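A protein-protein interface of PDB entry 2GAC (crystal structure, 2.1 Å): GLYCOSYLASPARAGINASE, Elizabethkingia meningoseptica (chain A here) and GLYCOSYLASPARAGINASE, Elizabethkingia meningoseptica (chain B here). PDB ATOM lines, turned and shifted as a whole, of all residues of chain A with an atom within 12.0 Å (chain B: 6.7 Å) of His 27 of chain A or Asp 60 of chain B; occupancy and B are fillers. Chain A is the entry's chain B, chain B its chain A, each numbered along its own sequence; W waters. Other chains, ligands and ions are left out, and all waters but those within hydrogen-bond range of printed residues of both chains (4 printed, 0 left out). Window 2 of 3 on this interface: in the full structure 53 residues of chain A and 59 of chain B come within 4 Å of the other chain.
The backbone carbonyl oxygen of Pro 57 of chain B is in hydrogen-bond range of the backbone NH of Tyr 24 of chain A. The side-chain carboxylate of Asp 58 of chain B sits at hydrogen-bond distance from a ring nitrogen (ND1) of His 27 of chain A (2.9 Å). The backbone NH (N) of Arg 59 of chain B is in hydrogen-bond range of the backbone carbonyl oxygen (O) of Lys 25 of chain A, 2.9 Å away. The side-chain amino group (NZ) of Lys 25 of chain A lies within hydrogen-bond range of the side-chain hydroxyl (OG1) of Thr 64 of chain B, at 2.7 Å. O of Thr 64 of chain B lies close to O of Ser 20 of chain A, at 3.4 Å.
Water W2 lies within hydrogen-bond range of the side-chain carboxylate (OD2) of Asp 60 of chain B (2.7 Å), the guanidinium group (NE) of Arg 59 of chain B (2.8 Å) and the backbone NH (N) of His 27 of chain A (3.1 Å). Water W3 lies within hydrogen-bond range of the backbone NH (N) of Gly 28 of chain A (2.7 Å), the side-chain carboxylate (OD2) of Asp 58 of chain B (2.8 Å) and the side-chain hydroxyl (OG1) of Thr 64 of chain B (3.0 Å). Water W4 lies within hydrogen-bond range of the side-chain hydroxyl of Thr 64 of chain B (2.9 Å), the backbone carbonyl oxygen of Arg 29 of chain A (2.9 Å) and the side-chain amino group of Lys 25 of chain A (3.0 Å). Water W1 lies within hydrogen-bond range of the backbone carbonyl oxygen (O) of Ser 20 of chain A (2.9 Å), the backbone NH (N) of Thr 64 of chain B (3.1 Å) and the side-chain amino group (NZ) of Lys 25 of chain A (3.4 Å).
Met 22 of chain A touches none of the printed residues of chain B. Printed residues of chain B within 4 Å of Ala 23 of chain A: Pro 57. Of the printed residues of chain B, Tyr 24 of chain A touches Pro 57 (2.8 Å), Asp 58 (3.6 Å), Arg 59 (3.5 Å), Trp 132 (3.6 Å) and Trp 135 (3.6 Å). Of the printed residues of chain B, Lys 25 of chain A touches Asp 58, Arg 59 and Thr 64. His 27 of chain A touches three residues of chain B. Printed residues of chain B within 4 Å of Gly 28 of chain A: Cys 81 (3.6 Å). Pro 57 of chain B touches two residues of chain A. Of the printed residues of chain A, Asp 58 of chain B touches Tyr 24, Lys 25 and His 27. Arg 59 of chain B touches just these residues of chain A: Tyr 24, Lys 25 and Met 26. Gly 61 of chain B touches none of the printed residues of chain A. Arg 62 of chain B touches one residue of chain A. Of the printed residues of chain A, Thr 64 of chain B touches Ser 20 and Lys 25. The nearest residue of chain A that does not touch Asp 60 of chain B is Lys 25 of chain A (5.1 Å). The nearest printed residue of chain B that does not touch Tyr 24 of chain A is Asp 60 of chain B (6.0 Å).
Among the printed residues, merely in contact across the chains: Lys 25 of chain A with Asp 58 of chain B (3.3 Å), Tyr 24 of chain A with Arg 59 of chain B (3.5 Å), His 27 of chain A with Asp 60 of chain B (3.5 Å), Tyr 24 of chain A with Asp 58 of chain B (3.6 Å), Tyr 24 of chain A with Trp 135 of chain B (3.6 Å), Tyr 24 of chain A with Trp 132 of chain B (3.6 Å), Gly 28 of chain A with Cys 81 of chain B (3.6 Å), Ala 23 of chain A with Pro 57 of chain B (3.7 Å), Met 26 of chain A with Arg 59 of chain B (3.8 Å) and His 27 of chain A with Arg 62 of chain B (3.8 Å).
Of the 12 printed residues of chain B, 9 touch a printed residue of chain A. Printed residues of chain B that touch a printed residue of chain A: Pro 57, Asp 58, Arg 59, Asp 60, Arg 62, Thr 64, Cys 81, Trp 132 and Trp 135. Hydrophobic or aromatic side chains of chain B that line the printed part of chain A: Trp 132 and Trp 135. Along chain B the printed residues that touch a printed residue of chain A span positions 57 to 135. Among the printed residues, 15 pairs touch across the chains. Among the printed residues, no Asp or Glu carboxylate lies within 4 Å of a Lys or Arg side-chain nitrogen of the other chain.
OD1 of Asp 58 of chain B lies close to N of Asp 60 of chain B. The side-chain carboxylate (OD1) of Asp 58 of chain B lies within hydrogen-bond range of the backbone NH (N) of Arg 62 of chain B (2.9 Å). The indole nitrogen of Trp 132 of chain B lies within hydrogen-bond range of the backbone carbonyl oxygen of Arg 59 of chain B, at 3.0 Å. The side-chain carboxylate of Glu 83 of chain B lies within salt-bridge range of the guanidinium group of Arg 62 of chain B (2.6 Å). The backbone carbonyl oxygen (O) of Ser 20 of chain A is in hydrogen-bond range of the side-chain amino group (NZ) of Lys 25 of chain A, at 2.9 Å.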
ATOM      1  N   SER A  20      28.245  23.327  -1.095  1.00  0.00           N
ATOM      2  CA  SER A  20      27.510  23.813   0.055  1.00  0.00           C
ATOM      3  C   SER A  20      27.223  22.640   1.011  1.00  0.00           C
ATOM      4  O   SER A  20      26.580  22.776   2.060  1.00  0.00           O
ATOM      5  CB  SER A  20      26.219  24.479  -0.407  1.00  0.00           C
ATOM      6  OG  SER A  20      25.539  23.792  -1.443  1.00  0.00           O
ATOM      7  N   GLY A  21      27.736  21.450   0.661  1.00  0.00           N
ATOM      8  CA  GLY A  21      27.630  20.258   1.477  1.00  0.00           C
ATOM      9  C   GLY A  21      26.252  19.619   1.460  1.00  0.00           C
ATOM     10  O   GLY A  21      25.388  19.948   0.651  1.00  0.00           O
ATOM     11  N   MET A  22      26.089  18.687   2.397  1.00  0.00           N
ATOM     12  CA  MET A  22      24.869  17.915   2.503  1.00  0.00           C
ATOM     13  C   MET A  22      23.773  18.847   2.981  1.00  0.00           C
ATOM     14  O   MET A  22      23.962  19.574   3.966  1.00  0.00           O
ATOM     15  CB  MET A  22      25.046  16.789   3.508  1.00  0.00           C
ATOM     16  CG  MET A  22      23.780  15.959   3.668  1.00  0.00           C
ATOM     17  SD  MET A  22      23.740  15.049   5.232  1.00  0.00           S
ATOM     18  CE  MET A  22      24.699  13.672   4.674  1.00  0.00           C
ATOM     19  N   ALA A  23      22.631  18.806   2.303  1.00  0.00           N
ATOM     20  CA  ALA A  23      21.534  19.669   2.688  1.00  0.00           C
ATOM     21  C   ALA A  23      21.013  19.226   4.040  1.00  0.00           C
ATOM     22  O   ALA A  23      20.877  18.040   4.333  1.00  0.00           O
ATOM     23  CB  ALA A  23      20.398  19.565   1.696  1.00  0.00           C
ATOM     24  N   TYR A  24      20.752  20.219   4.875  1.00  0.00           N
ATOM     25  CA  TYR A  24      20.229  20.070   6.230  1.00  0.00           C
ATOM     26  C   TYR A  24      21.123  19.242   7.135  1.00  0.00           C
ATOM     27  O   TYR A  24      20.686  18.648   8.124  1.00  0.00           O
ATOM     28  CB  TYR A  24      18.805  19.473   6.165  1.00  0.00           C
ATOM     29  CG  TYR A  24      17.988  20.167   5.083  1.00  0.00           C
ATOM     30  CD1 TYR A  24      17.897  21.558   5.063  1.00  0.00           C
ATOM     31  CD2 TYR A  24      17.442  19.409   4.049  1.00  0.00           C
ATOM     32  CE1 TYR A  24      17.276  22.195   3.995  1.00  0.00           C
ATOM     33  CE2 TYR A  24      16.814  20.044   2.978  1.00  0.00           C
ATOM     34  CZ  TYR A  24      16.743  21.436   2.957  1.00  0.00           C
ATOM     35  OH  TYR A  24      16.183  22.095   1.882  1.00  0.00           O
ATOM     36  N   LYS A  25      22.426  19.274   6.825  1.00  0.00           N
ATOM     37  CA  LYS A  25      23.484  18.667   7.622  1.00  0.00           C
ATOM     38  C   LYS A  25      23.487  19.296   9.010  1.00  0.00           C
ATOM     39  O   LYS A  25      22.895  20.363   9.213  1.00  0.00           O
ATOM     40  CB  LYS A  25      24.855  18.910   6.955  1.00  0.00           C
ATOM     41  CG  LYS A  25      25.271  20.401   6.866  1.00  0.00           C
ATOM     42  CD  LYS A  25      26.309  20.822   5.811  1.00  0.00           C
ATOM     43  CE  LYS A  25      26.360  22.360   5.804  1.00  0.00           C
ATOM     44  NZ  LYS A  25      27.238  23.008   4.835  1.00  0.00           N
ATOM     45  N   MET A  26      24.083  18.665  10.022  1.00  0.00           N
ATOM     46  CA  MET A  26      24.300  19.360  11.289  1.00  0.00           C
ATOM     47  C   MET A  26      25.188  20.578  11.068  1.00  0.00           C
ATOM     48  O   MET A  26      26.053  20.612  10.181  1.00  0.00           O
ATOM     49  CB  MET A  26      24.992  18.484  12.323  1.00  0.00           C
ATOM     50  CG  MET A  26      24.166  17.289  12.756  1.00  0.00           C
ATOM     51  SD  MET A  26      24.918  16.318  14.092  1.00  0.00           S
ATOM     52  CE  MET A  26      26.507  15.994  13.414  1.00  0.00           C
ATOM     53  N   HIS A  27      24.937  21.590  11.891  1.00  0.00           N
ATOM     54  CA  HIS A  27      25.712  22.808  11.841  1.00  0.00           C
ATOM     55  C   HIS A  27      27.173  22.491  12.145  1.00  0.00           C
ATOM     56  O   HIS A  27      27.486  21.794  13.114  1.00  0.00           O
ATOM     57  CB  HIS A  27      25.120  23.790  12.849  1.00  0.00           C
ATOM     58  CG  HIS A  27      25.852  25.118  12.846  1.00  0.00           C
ATOM     59  ND1 HIS A  27      26.184  25.887  11.818  1.00  0.00           N
ATOM     60  CD2 HIS A  27      26.347  25.696  13.979  1.00  0.00           C
ATOM     61  CE1 HIS A  27      26.876  26.899  12.303  1.00  0.00           C
ATOM     62  NE2 HIS A  27      26.969  26.775  13.611  1.00  0.00           N
ATOM     63  N   GLY A  28      28.090  22.980  11.322  1.00  0.00           N
ATOM     64  CA  GLY A  28      29.496  22.697  11.503  1.00  0.00           C
ATOM     65  C   GLY A  28      29.918  21.418  10.815  1.00  0.00           C
ATOM     66  O   GLY A  28      31.072  21.008  10.974  1.00  0.00           O
ATOM     67  N   ARG A  29      29.061  20.754  10.045  1.00  0.00           N
ATOM     68  CA  ARG A  29      29.467  19.540   9.389  1.00  0.00           C
ATOM     69  C   ARG A  29      30.326  19.893   8.179  1.00  0.00           C
ATOM     70  O   ARG A  29      30.012  20.784   7.385  1.00  0.00           O
ATOM     71  CB  ARG A  29      28.218  18.768   8.997  1.00  0.00           C
ATOM     72  CG  ARG A  29      28.408  17.482   8.228  1.00  0.00           C
ATOM     73  CD  ARG A  29      28.496  17.741   6.741  1.00  0.00           C
ATOM     74  NE  ARG A  29      28.622  16.529   5.984  1.00  0.00           N
ATOM     75  CZ  ARG A  29      28.791  16.550   4.663  1.00  0.00           C
ATOM     76  NH1 ARG A  29      28.865  17.726   4.012  1.00  0.00           N
ATOM     77  NH2 ARG A  29      28.851  15.364   4.033  1.00  0.00           N
ATOM     78  N   VAL A  30      31.388  19.126   8.006  1.00  0.00           N
ATOM     79  CA  VAL A  30      32.282  19.319   6.890  1.00  0.00           C
ATOM     80  C   VAL A  30      32.398  17.977   6.153  1.00  0.00           C
ATOM     81  O   VAL A  30      32.413  16.907   6.775  1.00  0.00           O
ATOM     82  CB  VAL A  30      33.622  19.828   7.486  1.00  0.00           C
ATOM     83  CG1 VAL A  30      34.668  19.904   6.398  1.00  0.00           C
ATOM     84  CG2 VAL A  30      33.451  21.229   8.080  1.00  0.00           C
ATOM     85  N   GLY A  31      32.362  17.997   4.819  1.00  0.00           N
ATOM     86  CA  GLY A  31      32.520  16.784   4.026  1.00  0.00           C
ATOM     87  C   GLY A  31      33.920  16.707   3.410  1.00  0.00           C
ATOM     88  O   GLY A  31      34.867  17.337   3.879  1.00  0.00           O
ATOM     89  N   GLU A  56      31.264  11.754   3.836  1.00  0.00           N
ATOM     90  CA  GLU A  56      31.713  10.899   4.928  1.00  0.00           C
ATOM     91  C   GLU A  56      32.530   9.707   4.466  1.00  0.00           C
ATOM     92  O   GLU A  56      33.601   9.396   5.011  1.00  0.00           O
ATOM     93  CB  GLU A  56      30.491  10.396   5.722  1.00  0.00           C
ATOM     94  CG  GLU A  56      29.742  11.405   6.620  1.00  0.00           C
ATOM     95  CD  GLU A  56      29.056  12.604   5.963  1.00  0.00           C
ATOM     96  OE1 GLU A  56      28.735  12.595   4.779  1.00  0.00           O
ATOM     97  OE2 GLU A  56      28.839  13.614   6.620  1.00  0.00           O
ATOM     98  N   PRO B  57      20.970  25.037   2.754  1.00  0.00           N
ATOM     99  CA  PRO B  57      21.552  25.260   4.073  1.00  0.00           C
ATOM    100  C   PRO B  57      21.658  24.023   4.945  1.00  0.00           C
ATOM    101  O   PRO B  57      21.196  22.930   4.568  1.00  0.00           O
ATOM    102  CB  PRO B  57      20.660  26.337   4.636  1.00  0.00           C
ATOM    103  CG  PRO B  57      19.295  25.987   4.113  1.00  0.00           C
ATOM    104  CD  PRO B  57      19.627  25.612   2.681  1.00  0.00           C
ATOM    105  N   ASP B  58      22.284  24.196   6.105  1.00  0.00           N
ATOM    106  CA  ASP B  58      22.337  23.164   7.120  1.00  0.00           C
ATOM    107  C   ASP B  58      20.995  23.179   7.852  1.00  0.00           C
ATOM    108  O   ASP B  58      20.092  23.973   7.548  1.00  0.00           O
ATOM    109  CB  ASP B  58      23.527  23.405   8.114  1.00  0.00           C
ATOM    110  CG  ASP B  58      23.607  24.651   8.989  1.00  0.00           C
ATOM    111  OD1 ASP B  58      22.600  25.298   9.245  1.00  0.00           O
ATOM    112  OD2 ASP B  58      24.699  24.983   9.458  1.00  0.00           O
ATOM    113  N   ARG B  59      20.834  22.306   8.841  1.00  0.00           N
ATOM    114  CA  ARG B  59      19.548  22.141   9.480  1.00  0.00           C
ATOM    115  C   ARG B  59      19.036  23.374  10.177  1.00  0.00           C
ATOM    116  O   ARG B  59      17.815  23.527  10.332  1.00  0.00           O
ATOM    117  CB  ARG B  59      19.608  20.954  10.461  1.00  0.00           C
ATOM    118  CG  ARG B  59      20.612  20.926  11.601  1.00  0.00           C
ATOM    119  CD  ARG B  59      20.649  19.515  12.183  1.00  0.00           C
ATOM    120  NE  ARG B  59      21.159  19.526  13.542  1.00  0.00           N
ATOM    121  CZ  ARG B  59      20.924  18.554  14.441  1.00  0.00           C
ATOM    122  NH1 ARG B  59      20.176  17.494  14.106  1.00  0.00           N
ATOM    123  NH2 ARG B  59      21.411  18.695  15.684  1.00  0.00           N
ATOM    124  N   ASP B  60      19.924  24.330  10.442  1.00  0.00           N
ATOM    125  CA  ASP B  60      19.499  25.518  11.147  1.00  0.00           C
ATOM    126  C   ASP B  60      19.380  26.694  10.199  1.00  0.00           C
ATOM    127  O   ASP B  60      19.335  27.869  10.573  1.00  0.00           O
ATOM    128  CB  ASP B  60      20.509  25.753  12.263  1.00  0.00           C
ATOM    129  CG  ASP B  60      20.564  24.567  13.212  1.00  0.00           C
ATOM    130  OD1 ASP B  60      19.534  24.065  13.662  1.00  0.00           O
ATOM    131  OD2 ASP B  60      21.655  24.085  13.476  1.00  0.00           O
ATOM    132  N   GLY B  61      19.271  26.351   8.919  1.00  0.00           N
ATOM    133  CA  GLY B  61      19.086  27.328   7.875  1.00  0.00           C
ATOM    134  C   GLY B  61      20.303  28.167   7.611  1.00  0.00           C
ATOM    135  O   GLY B  61      20.161  29.248   7.042  1.00  0.00           O
ATOM    136  N   ARG B  62      21.508  27.717   7.959  1.00  0.00           N
ATOM    137  CA  ARG B  62      22.702  28.492   7.670  1.00  0.00           C
ATOM    138  C   ARG B  62      23.419  27.900   6.456  1.00  0.00           C
ATOM    139  O   ARG B  62      23.658  26.692   6.379  1.00  0.00           O
ATOM    140  CB  ARG B  62      23.624  28.488   8.881  1.00  0.00           C
ATOM    141  CG  ARG B  62      22.931  28.985  10.145  1.00  0.00           C
ATOM    142  CD  ARG B  62      23.907  29.134  11.301  1.00  0.00           C
ATOM    143  NE  ARG B  62      24.789  30.260  11.052  1.00  0.00           N
ATOM    144  CZ  ARG B  62      25.458  30.935  12.002  1.00  0.00           C
ATOM    145  NH1 ARG B  62      25.383  30.618  13.309  1.00  0.00           N
ATOM    146  NH2 ARG B  62      26.148  32.008  11.617  1.00  0.00           N
ATOM    147  N   THR B  64      26.656  27.046   4.686  1.00  0.00           N
ATOM    148  CA  THR B  64      28.065  27.116   5.041  1.00  0.00           C
ATOM    149  C   THR B  64      28.781  26.324   3.957  1.00  0.00           C
ATOM    150  O   THR B  64      28.393  25.187   3.658  1.00  0.00           O
ATOM    151  CB  THR B  64      28.247  26.511   6.456  1.00  0.00           C
ATOM    152  OG1 THR B  64      27.871  25.142   6.341  1.00  0.00           O
ATOM    153  CG2 THR B  64      27.386  27.168   7.542  1.00  0.00           C
ATOM    154  N   CYS B  81      33.173  25.296   6.230  1.00  0.00           N
ATOM    155  CA  CYS B  81      32.102  25.836   7.051  1.00  0.00           C
ATOM    156  C   CYS B  81      32.226  27.350   7.173  1.00  0.00           C
ATOM    157  O   CYS B  81      32.183  27.966   8.242  1.00  0.00           O
ATOM    158  CB  CYS B  81      32.115  25.177   8.434  1.00  0.00           C
ATOM    159  SG  CYS B  81      30.556  25.408   9.325  1.00  0.00           S
ATOM    160  N   GLU B  83      30.648  31.004   6.003  1.00  0.00           N
ATOM    161  CA  GLU B  83      29.381  31.577   5.626  1.00  0.00           C
ATOM    162  C   GLU B  83      29.563  32.876   4.861  1.00  0.00           C
ATOM    163  O   GLU B  83      30.603  33.522   4.949  1.00  0.00           O
ATOM    164  CB  GLU B  83      28.576  31.877   6.852  1.00  0.00           C
ATOM    165  CG  GLU B  83      27.465  30.894   7.017  1.00  0.00           C
ATOM    166  CD  GLU B  83      26.444  31.344   8.018  1.00  0.00           C
ATOM    167  OE1 GLU B  83      26.718  31.228   9.198  1.00  0.00           O
ATOM    168  OE2 GLU B  83      25.376  31.831   7.644  1.00  0.00           O
ATOM    169  N   TRP B 132      13.849  24.646   2.889  1.00  0.00           N
ATOM    170  CA  TRP B 132      14.361  24.363   4.224  1.00  0.00           C
ATOM    171  C   TRP B 132      13.200  24.300   5.199  1.00  0.00           C
ATOM    172  O   TRP B 132      13.054  23.332   5.948  1.00  0.00           O
ATOM    173  CB  TRP B 132      15.373  25.453   4.648  1.00  0.00           C
ATOM    174  CG  TRP B 132      15.742  25.487   6.133  1.00  0.00           C
ATOM    175  CD1 TRP B 132      16.199  24.389   6.826  1.00  0.00           C
ATOM    176  CD2 TRP B 132      15.593  26.583   6.931  1.00  0.00           C
ATOM    177  NE1 TRP B 132      16.323  24.794   8.067  1.00  0.00           N
ATOM    178  CE2 TRP B 132      15.976  26.083   8.180  1.00  0.00           C
ATOM    179  CE3 TRP B 132      15.192  27.908   6.785  1.00  0.00           C
ATOM    180  CZ2 TRP B 132      15.958  26.908   9.304  1.00  0.00           C
ATOM    181  CZ3 TRP B 132      15.179  28.731   7.907  1.00  0.00           C
ATOM    182  CH2 TRP B 132      15.556  28.238   9.157  1.00  0.00           C
ATOM    183  N   TRP B 135      11.222  21.208   4.739  1.00  0.00           N
ATOM    184  CA  TRP B 135      11.919  20.114   5.418  1.00  0.00           C
ATOM    185  C   TRP B 135      11.741  20.194   6.938  1.00  0.00           C
ATOM    186  O   TRP B 135      11.611  19.158   7.589  1.00  0.00           O
ATOM    187  CB  TRP B 135      13.426  20.153   5.072  1.00  0.00           C
ATOM    188  CG  TRP B 135      14.293  19.131   5.807  1.00  0.00           C
ATOM    189  CD1 TRP B 135      14.376  17.834   5.375  1.00  0.00           C
ATOM    190  CD2 TRP B 135      15.031  19.353   6.951  1.00  0.00           C
ATOM    191  NE1 TRP B 135      15.155  17.232   6.239  1.00  0.00           N
ATOM    192  CE2 TRP B 135      15.560  18.081   7.192  1.00  0.00           C
ATOM    193  CE3 TRP B 135      15.319  20.406   7.819  1.00  0.00           C
ATOM    194  CZ2 TRP B 135      16.393  17.841   8.286  1.00  0.00           C
ATOM    195  CZ3 TRP B 135      16.151  20.172   8.919  1.00  0.00           C
ATOM    196  CH2 TRP B 135      16.679  18.899   9.154  1.00  0.00           C
ATOM    197  N   LEU B 136      11.731  21.383   7.546  1.00  0.00           N
ATOM    198  CA  LEU B 136      11.521  21.510   8.979  1.00  0.00           C
ATOM    199  C   LEU B 136      10.147  20.976   9.377  1.00  0.00           C
ATOM    200  O   LEU B 136       9.979  20.449  10.475  1.00  0.00           O
ATOM    201  CB  LEU B 136      11.635  22.974   9.412  1.00  0.00           C
ATOM    202  CG  LEU B 136      12.962  23.715   9.330  1.00  0.00           C
ATOM    203  CD1 LEU B 136      12.759  25.122   9.856  1.00  0.00           C
ATOM    204  CD2 LEU B 136      14.023  23.031  10.176  1.00  0.00           C
HETATM  205  O   HOH W   1      24.996  24.904   3.192  1.00  0.00           O
HETATM  206  O   HOH W   2      22.761  21.730  14.147  1.00  0.00           O
HETATM  207  O   HOH W   3      27.127  23.700   8.871  1.00  0.00           O
HETATM  208  O   HOH W   4      30.032  23.288   5.897  1.00  0.00           O
